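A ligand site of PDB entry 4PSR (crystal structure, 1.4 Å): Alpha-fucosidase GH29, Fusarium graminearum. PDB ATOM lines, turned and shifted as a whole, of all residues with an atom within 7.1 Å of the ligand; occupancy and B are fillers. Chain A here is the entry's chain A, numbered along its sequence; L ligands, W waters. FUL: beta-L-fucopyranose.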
ATOM      1  N   TYR A  32       4.267 -37.987 -26.348  1.00  0.00           N
ATOM      2  CA  TYR A  32       5.368 -37.794 -25.412  1.00  0.00           C
ATOM      3  C   TYR A  32       4.829 -37.457 -24.036  1.00  0.00           C
ATOM      4  O   TYR A  32       3.620 -37.359 -23.845  1.00  0.00           O
ATOM      5  CB  TYR A  32       6.437 -36.791 -25.894  1.00  0.00           C
ATOM      6  CG  TYR A  32       6.176 -35.287 -25.895  1.00  0.00           C
ATOM      7  CD1 TYR A  32       7.227 -34.411 -25.684  1.00  0.00           C
ATOM      8  CD2 TYR A  32       4.935 -34.747 -26.174  1.00  0.00           C
ATOM      9  CE1 TYR A  32       7.054 -33.061 -25.723  1.00  0.00           C
ATOM     10  CE2 TYR A  32       4.743 -33.371 -26.205  1.00  0.00           C
ATOM     11  CZ  TYR A  32       5.810 -32.544 -25.998  1.00  0.00           C
ATOM     12  OH  TYR A  32       5.590 -31.162 -26.074  1.00  0.00           O
ATOM     13  N   HIS A  34       5.621 -35.257 -20.283  1.00  0.00           N
ATOM     14  CA  HIS A  34       6.306 -34.391 -19.341  1.00  0.00           C
ATOM     15  C   HIS A  34       6.255 -35.040 -17.956  1.00  0.00           C
ATOM     16  O   HIS A  34       5.361 -34.761 -17.161  1.00  0.00           O
ATOM     17  CB  HIS A  34       5.639 -33.003 -19.283  1.00  0.00           C
ATOM     18  CG  HIS A  34       5.958 -32.107 -20.436  1.00  0.00           C
ATOM     19  ND1 HIS A  34       5.564 -32.351 -21.741  1.00  0.00           N
ATOM     20  CD2 HIS A  34       6.609 -30.905 -20.466  1.00  0.00           C
ATOM     21  CE1 HIS A  34       5.973 -31.352 -22.509  1.00  0.00           C
ATOM     22  NE2 HIS A  34       6.602 -30.473 -21.760  1.00  0.00           N
ATOM     23  N   SER A  45       2.119 -26.493 -12.213  1.00  0.00           N
ATOM     24  CA  SER A  45       2.558 -26.952 -13.524  1.00  0.00           C
ATOM     25  C   SER A  45       3.979 -27.439 -13.455  1.00  0.00           C
ATOM     26  O   SER A  45       4.629 -27.422 -12.398  1.00  0.00           O
ATOM     27  CB  SER A  45       2.482 -25.821 -14.557  1.00  0.00           C
ATOM     28  OG  SER A  45       3.477 -24.864 -14.284  1.00  0.00           O
ATOM     29  N   GLU A  46       4.461 -27.897 -14.604  1.00  0.00           N
ATOM     30  CA  GLU A  46       5.866 -28.252 -14.762  1.00  0.00           C
ATOM     31  C   GLU A  46       6.823 -27.072 -14.584  1.00  0.00           C
ATOM     32  O   GLU A  46       8.025 -27.295 -14.499  1.00  0.00           O
ATOM     33  CB  GLU A  46       6.082 -28.919 -16.128  1.00  0.00           C
ATOM     34  CG  GLU A  46       6.026 -27.993 -17.345  1.00  0.00           C
ATOM     35  CD  GLU A  46       4.668 -27.423 -17.700  1.00  0.00           C
ATOM     36  OE1 GLU A  46       3.613 -27.934 -17.276  1.00  0.00           O
ATOM     37  OE2 GLU A  46       4.664 -26.408 -18.447  1.00  0.00           O
ATOM     38  N   TRP A  47       6.303 -25.827 -14.528  1.00  0.00           N
ATOM     39  CA  TRP A  47       7.135 -24.672 -14.181  1.00  0.00           C
ATOM     40  C   TRP A  47       7.307 -24.488 -12.661  1.00  0.00           C
ATOM     41  O   TRP A  47       7.939 -23.537 -12.234  1.00  0.00           O
ATOM     42  CB  TRP A  47       6.635 -23.367 -14.840  1.00  0.00           C
ATOM     43  CG  TRP A  47       7.031 -23.234 -16.282  1.00  0.00           C
ATOM     44  CD1 TRP A  47       7.210 -24.231 -17.218  1.00  0.00           C
ATOM     45  CD2 TRP A  47       7.328 -21.999 -16.977  1.00  0.00           C
ATOM     46  NE1 TRP A  47       7.601 -23.696 -18.425  1.00  0.00           N
ATOM     47  CE2 TRP A  47       7.691 -22.323 -18.299  1.00  0.00           C
ATOM     48  CE3 TRP A  47       7.311 -20.649 -16.589  1.00  0.00           C
ATOM     49  CZ2 TRP A  47       8.053 -21.344 -19.238  1.00  0.00           C
ATOM     50  CZ3 TRP A  47       7.683 -19.681 -17.525  1.00  0.00           C
ATOM     51  CH2 TRP A  47       8.053 -20.029 -18.824  1.00  0.00           C
ATOM     52  N   VAL A 123      10.091 -36.592 -22.488  1.00  0.00           N
ATOM     53  CA  VAL A 123      10.892 -35.422 -22.184  1.00  0.00           C
ATOM     54  C   VAL A 123      12.131 -35.956 -21.466  1.00  0.00           C
ATOM     55  O   VAL A 123      12.037 -36.552 -20.392  1.00  0.00           O
ATOM     56  CB  VAL A 123      10.125 -34.410 -21.293  1.00  0.00           C
ATOM     57  CG1 VAL A 123      11.062 -33.344 -20.755  1.00  0.00           C
ATOM     58  CG2 VAL A 123       8.986 -33.794 -22.077  1.00  0.00           C
ATOM     59  N   HIS A 126      13.819 -31.229 -19.156  1.00  0.00           N
ATOM     60  CA  HIS A 126      13.000 -30.035 -19.302  1.00  0.00           C
ATOM     61  C   HIS A 126      13.865 -28.789 -19.015  1.00  0.00           C
ATOM     62  O   HIS A 126      15.033 -28.799 -19.350  1.00  0.00           O
ATOM     63  CB  HIS A 126      11.741 -30.170 -18.426  1.00  0.00           C
ATOM     64  CG  HIS A 126      10.641 -29.259 -18.837  1.00  0.00           C
ATOM     65  ND1 HIS A 126      10.358 -28.100 -18.143  1.00  0.00           N
ATOM     66  CD2 HIS A 126       9.811 -29.280 -19.901  1.00  0.00           C
ATOM     67  CE1 HIS A 126       9.369 -27.461 -18.743  1.00  0.00           C
ATOM     68  NE2 HIS A 126       9.020 -28.154 -19.816  1.00  0.00           N
ATOM     69  N   HIS A 127      13.291 -27.717 -18.452  1.00  0.00           N
ATOM     70  CA  HIS A 127      14.038 -26.491 -18.157  1.00  0.00           C
ATOM     71  C   HIS A 127      14.761 -26.551 -16.799  1.00  0.00           C
ATOM     72  O   HIS A 127      15.536 -25.643 -16.499  1.00  0.00           O
ATOM     73  CB  HIS A 127      13.101 -25.258 -18.041  1.00  0.00           C
ATOM     74  CG  HIS A 127      12.233 -24.956 -19.232  1.00  0.00           C
ATOM     75  ND1 HIS A 127      12.650 -25.013 -20.555  1.00  0.00           N
ATOM     76  CD2 HIS A 127      10.953 -24.500 -19.258  1.00  0.00           C
ATOM     77  CE1 HIS A 127      11.649 -24.596 -21.328  1.00  0.00           C
ATOM     78  NE2 HIS A 127      10.610 -24.309 -20.573  1.00  0.00           N
ATOM     79  N   HIS A 171      14.565 -29.398 -23.423  1.00  0.00           N
ATOM     80  CA  HIS A 171      14.159 -28.019 -23.148  1.00  0.00           C
ATOM     81  C   HIS A 171      15.266 -27.292 -22.325  1.00  0.00           C
ATOM     82  O   HIS A 171      14.975 -26.434 -21.493  1.00  0.00           O
ATOM     83  CB  HIS A 171      12.809 -27.926 -22.379  1.00  0.00           C
ATOM     84  CG  HIS A 171      11.735 -28.898 -22.781  1.00  0.00           C
ATOM     85  ND1 HIS A 171      10.429 -28.500 -23.026  1.00  0.00           N
ATOM     86  CD2 HIS A 171      11.736 -30.256 -22.912  1.00  0.00           C
ATOM     87  CE1 HIS A 171       9.680 -29.559 -23.280  1.00  0.00           C
ATOM     88  NE2 HIS A 171      10.445 -30.631 -23.211  1.00  0.00           N
ATOM     89  N   TYR A 174      16.422 -22.884 -21.861  1.00  0.00           N
ATOM     90  CA  TYR A 174      15.870 -21.860 -20.974  1.00  0.00           C
ATOM     91  C   TYR A 174      16.395 -22.016 -19.551  1.00  0.00           C
ATOM     92  O   TYR A 174      16.402 -21.066 -18.750  1.00  0.00           O
ATOM     93  CB  TYR A 174      14.334 -21.859 -21.033  1.00  0.00           C
ATOM     94  CG  TYR A 174      13.644 -20.781 -20.245  1.00  0.00           C
ATOM     95  CD1 TYR A 174      14.118 -19.459 -20.236  1.00  0.00           C
ATOM     96  CD2 TYR A 174      12.470 -21.056 -19.571  1.00  0.00           C
ATOM     97  CE1 TYR A 174      13.459 -18.495 -19.526  1.00  0.00           C
ATOM     98  CE2 TYR A 174      11.802 -20.074 -18.849  1.00  0.00           C
ATOM     99  CZ  TYR A 174      12.291 -18.791 -18.843  1.00  0.00           C
ATOM    100  OH  TYR A 174      11.588 -17.848 -18.108  1.00  0.00           O
ATOM    101  N   PHE A 179      14.988 -19.390 -16.583  1.00  0.00           N
ATOM    102  CA  PHE A 179      14.041 -20.235 -15.841  1.00  0.00           C
ATOM    103  C   PHE A 179      14.228 -20.148 -14.343  1.00  0.00           C
ATOM    104  O   PHE A 179      13.260 -20.024 -13.603  1.00  0.00           O
ATOM    105  CB  PHE A 179      14.204 -21.683 -16.295  1.00  0.00           C
ATOM    106  CG  PHE A 179      13.167 -22.646 -15.737  1.00  0.00           C
ATOM    107  CD1 PHE A 179      11.858 -22.618 -16.186  1.00  0.00           C
ATOM    108  CD2 PHE A 179      13.533 -23.608 -14.805  1.00  0.00           C
ATOM    109  CE1 PHE A 179      10.909 -23.528 -15.713  1.00  0.00           C
ATOM    110  CE2 PHE A 179      12.591 -24.525 -14.342  1.00  0.00           C
ATOM    111  CZ  PHE A 179      11.293 -24.474 -14.788  1.00  0.00           C
ATOM    112  N   TRP A 224      13.311 -33.081 -30.352  1.00  0.00           N
ATOM    113  CA  TRP A 224      12.412 -31.953 -30.205  1.00  0.00           C
ATOM    114  C   TRP A 224      13.093 -30.959 -29.288  1.00  0.00           C
ATOM    115  O   TRP A 224      13.611 -31.345 -28.231  1.00  0.00           O
ATOM    116  CB  TRP A 224      11.116 -32.504 -29.625  1.00  0.00           C
ATOM    117  CG  TRP A 224       9.956 -31.594 -29.332  1.00  0.00           C
ATOM    118  CD1 TRP A 224       8.754 -31.594 -29.994  1.00  0.00           C
ATOM    119  CD2 TRP A 224       9.812 -30.654 -28.259  1.00  0.00           C
ATOM    120  NE1 TRP A 224       7.881 -30.729 -29.400  1.00  0.00           N
ATOM    121  CE2 TRP A 224       8.495 -30.116 -28.350  1.00  0.00           C
ATOM    122  CE3 TRP A 224      10.666 -30.192 -27.250  1.00  0.00           C
ATOM    123  CZ2 TRP A 224       8.017 -29.142 -27.464  1.00  0.00           C
ATOM    124  CZ3 TRP A 224      10.190 -29.197 -26.368  1.00  0.00           C
ATOM    125  CH2 TRP A 224       8.874 -28.692 -26.495  1.00  0.00           C
ATOM    126  N   ASP A 226      12.877 -27.028 -27.281  1.00  0.00           N
ATOM    127  CA  ASP A 226      12.084 -25.903 -26.824  1.00  0.00           C
ATOM    128  C   ASP A 226      12.789 -24.566 -27.143  1.00  0.00           C
ATOM    129  O   ASP A 226      13.868 -24.562 -27.694  1.00  0.00           O
ATOM    130  CB  ASP A 226      11.789 -26.025 -25.316  1.00  0.00           C
ATOM    131  CG  ASP A 226      10.448 -25.444 -24.920  1.00  0.00           C
ATOM    132  OD1 ASP A 226       9.875 -24.662 -25.743  1.00  0.00           O
ATOM    133  OD2 ASP A 226       9.970 -25.739 -23.826  1.00  0.00           O
ATOM    134  N   PHE A 227      12.125 -23.488 -26.760  1.00  0.00           N
ATOM    135  CA  PHE A 227      12.525 -22.113 -27.087  1.00  0.00           C
ATOM    136  C   PHE A 227      13.805 -21.698 -26.370  1.00  0.00           C
ATOM    137  O   PHE A 227      14.383 -22.460 -25.587  1.00  0.00           O
ATOM    138  CB  PHE A 227      11.387 -21.135 -26.755  1.00  0.00           C
ATOM    139  CG  PHE A 227      11.287 -20.771 -25.300  1.00  0.00           C
ATOM    140  CD1 PHE A 227      11.703 -19.533 -24.860  1.00  0.00           C
ATOM    141  CD2 PHE A 227      10.777 -21.647 -24.360  1.00  0.00           C
ATOM    142  CE1 PHE A 227      11.627 -19.174 -23.506  1.00  0.00           C
ATOM    143  CE2 PHE A 227      10.687 -21.297 -23.019  1.00  0.00           C
ATOM    144  CZ  PHE A 227      11.113 -20.045 -22.592  1.00  0.00           C
ATOM    145  N   LYS A 272      10.729 -24.441 -31.772  1.00  0.00           N
ATOM    146  CA  LYS A 272       9.492 -23.652 -31.680  1.00  0.00           C
ATOM    147  C   LYS A 272       9.381 -22.664 -32.839  1.00  0.00           C
ATOM    148  O   LYS A 272      10.348 -22.006 -33.190  1.00  0.00           O
ATOM    149  CB  LYS A 272       9.345 -22.973 -30.323  1.00  0.00           C
ATOM    150  CG  LYS A 272       9.190 -23.946 -29.176  1.00  0.00           C
ATOM    151  CD  LYS A 272       7.878 -24.749 -29.286  1.00  0.00           C
ATOM    152  CE  LYS A 272       7.640 -25.662 -28.091  1.00  0.00           C
ATOM    153  NZ  LYS A 272       7.303 -24.876 -26.878  1.00  0.00           N
ATOM    154  N   HIS A 274       8.214 -19.723 -33.434  1.00  0.00           N
ATOM    155  CA  HIS A 274       8.540 -18.296 -33.256  1.00  0.00           C
ATOM    156  C   HIS A 274      10.036 -18.056 -33.004  1.00  0.00           C
ATOM    157  O   HIS A 274      10.528 -16.938 -33.090  1.00  0.00           O
ATOM    158  CB  HIS A 274       7.718 -17.731 -32.117  1.00  0.00           C
ATOM    159  CG  HIS A 274       8.076 -18.308 -30.779  1.00  0.00           C
ATOM    160  ND1 HIS A 274       9.009 -17.734 -29.943  1.00  0.00           N
ATOM    161  CD2 HIS A 274       7.611 -19.404 -30.123  1.00  0.00           C
ATOM    162  CE1 HIS A 274       9.106 -18.434 -28.827  1.00  0.00           C
ATOM    163  NE2 HIS A 274       8.270 -19.451 -28.912  1.00  0.00           N
ATOM    164  N   ASP A 286       7.683 -26.107 -34.972  1.00  0.00           N
ATOM    165  CA  ASP A 286       6.727 -26.661 -34.010  1.00  0.00           C
ATOM    166  C   ASP A 286       5.851 -25.527 -33.508  1.00  0.00           C
ATOM    167  O   ASP A 286       6.288 -24.633 -32.768  1.00  0.00           O
ATOM    168  CB  ASP A 286       7.495 -27.338 -32.877  1.00  0.00           C
ATOM    169  CG  ASP A 286       6.612 -27.993 -31.882  1.00  0.00           C
ATOM    170  OD1 ASP A 286       6.956 -27.934 -30.664  1.00  0.00           O
ATOM    171  OD2 ASP A 286       5.596 -28.586 -32.269  1.00  0.00           O
ATOM    172  N   ASP A 303       2.345 -29.380 -30.799  1.00  0.00           N
ATOM    173  CA  ASP A 303       2.157 -30.213 -29.604  1.00  0.00           C
ATOM    174  C   ASP A 303       0.800 -29.929 -28.957  1.00  0.00           C
ATOM    175  O   ASP A 303       0.337 -28.789 -28.946  1.00  0.00           O
ATOM    176  CB  ASP A 303       3.248 -29.971 -28.568  1.00  0.00           C
ATOM    177  CG  ASP A 303       4.595 -29.816 -29.192  1.00  0.00           C
ATOM    178  OD1 ASP A 303       5.062 -30.761 -29.844  1.00  0.00           O
ATOM    179  OD2 ASP A 303       5.164 -28.694 -29.064  1.00  0.00           O
ATOM    180  N   TRP A 311       1.209 -29.293 -18.410  1.00  0.00           N
ATOM    181  CA  TRP A 311       1.803 -30.422 -19.171  1.00  0.00           C
ATOM    182  C   TRP A 311       2.169 -31.589 -18.244  1.00  0.00           C
ATOM    183  O   TRP A 311       2.288 -32.737 -18.681  1.00  0.00           O
ATOM    184  CB  TRP A 311       3.043 -29.979 -19.997  1.00  0.00           C
ATOM    185  CG  TRP A 311       2.724 -28.915 -20.989  1.00  0.00           C
ATOM    186  CD1 TRP A 311       2.635 -27.586 -20.740  1.00  0.00           C
ATOM    187  CD2 TRP A 311       2.441 -29.089 -22.394  1.00  0.00           C
ATOM    188  NE1 TRP A 311       2.308 -26.914 -21.882  1.00  0.00           N
ATOM    189  CE2 TRP A 311       2.188 -27.809 -22.916  1.00  0.00           C
ATOM    190  CE3 TRP A 311       2.393 -30.186 -23.261  1.00  0.00           C
ATOM    191  CZ2 TRP A 311       1.879 -27.586 -24.259  1.00  0.00           C
ATOM    192  CZ3 TRP A 311       2.102 -29.973 -24.595  1.00  0.00           C
ATOM    193  CH2 TRP A 311       1.832 -28.694 -25.078  1.00  0.00           C
ATOM    194  N   ASN A 342       0.879 -34.807 -25.651  1.00  0.00           N
ATOM    195  CA  ASN A 342       1.486 -34.979 -24.340  1.00  0.00           C
ATOM    196  C   ASN A 342       0.563 -35.650 -23.341  1.00  0.00           C
ATOM    197  O   ASN A 342      -0.623 -35.276 -23.260  1.00  0.00           O
ATOM    198  CB  ASN A 342       1.951 -33.630 -23.762  1.00  0.00           C
ATOM    199  CG  ASN A 342       2.430 -33.747 -22.360  1.00  0.00           C
ATOM    200  OD1 ASN A 342       3.539 -34.201 -22.138  1.00  0.00           O
ATOM    201  ND2 ASN A 342       1.621 -33.346 -21.409  1.00  0.00           N
HETATM  202  C1  FUL L   1       6.869 -24.682 -23.444  1.00  0.00           C
HETATM  203  C2  FUL L   1       7.457 -25.041 -22.094  1.00  0.00           C
HETATM  204  O2  FUL L   1       7.855 -23.885 -21.346  1.00  0.00           O
HETATM  205  C3  FUL L   1       6.384 -25.799 -21.365  1.00  0.00           C
HETATM  206  O3  FUL L   1       6.839 -26.103 -20.070  1.00  0.00           O
HETATM  207  C4  FUL L   1       6.105 -27.051 -22.159  1.00  0.00           C
HETATM  208  O4  FUL L   1       7.258 -27.880 -22.172  1.00  0.00           O
HETATM  209  C5  FUL L   1       5.691 -26.662 -23.576  1.00  0.00           C
HETATM  210  C6  FUL L   1       5.458 -27.865 -24.463  1.00  0.00           C
HETATM  211  O5  FUL L   1       6.649 -25.838 -24.214  1.00  0.00           O
HETATM  212  O1  FUL L   1       7.803 -23.891 -24.136  1.00  0.00           O
HETATM  213  O   HOH W   1       6.331 -21.445 -22.026  1.00  0.00           O
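An oxygen (O4) of the ligand is in hydrogen-bond range of a ring nitrogen (NE2) of His 34.
O3 of the ligand is in hydrogen-bond range of OE2 of Glu 46, 2.7 Å away.
OD1 of Asp 226 sits at hydrogen-bond distance from O1 of the ligand.
NE2 of His 127 lies within hydrogen-bond range of O2 of the ligand (2.9 Å).
The side-chain amino group (NZ) of Lys 272 sits at hydrogen-bond distance from an oxygen (O5) of the ligand.
O2 of the ligand sits at hydrogen-bond distance from NE1 of Trp 47 (2.9 Å).
NE2 of His 126 lies within hydrogen-bond range of O4 of the ligand, 3.0 Å away.
An oxygen (O4) of the ligand sits close to a ring nitrogen (ND1) of His 171 (3.3 Å).
A ring nitrogen (ND1) of His 34 lies within hydrogen-bond range of the side-chain amide oxygen of Asn 342.
The side-chain carboxylate (OE1) of Glu 46 sits at hydrogen-bond distance from the backbone NH (N) of Trp 311, at 3.0 Å.
OD1 of Asp 226 is in salt-bridge range of NZ of Lys 272, at 2.8 Å.
The side-chain carboxylate of Asp 226 is in hydrogen-bond range of a ring nitrogen (ND1) of His 171 (2.9 Å).
A ring nitrogen (ND1) of His 127 lies within hydrogen-bond range of the backbone carbonyl oxygen (O) of His 171, 2.9 Å away.
N of Trp 47 sits at hydrogen-bond distance from OG of Ser 45, at 3.0 Å.
The backbone carbonyl oxygen (O) of Trp 311 lies within hydrogen-bond range of the side-chain amide nitrogen (ND2) of Asn 342 (2.9 Å).
OH of Tyr 32 touches C6 of the ligand, at 3.7 Å.
Phe 227 touches the ligand (CD2 to O1, 3.7 Å).
Trp 311 touches the ligand.
Hydrophobic or aromatic side chains that line the ligand: His 34, Trp 47, His 126, His 127, His 171, Phe 227 and Trp 311.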
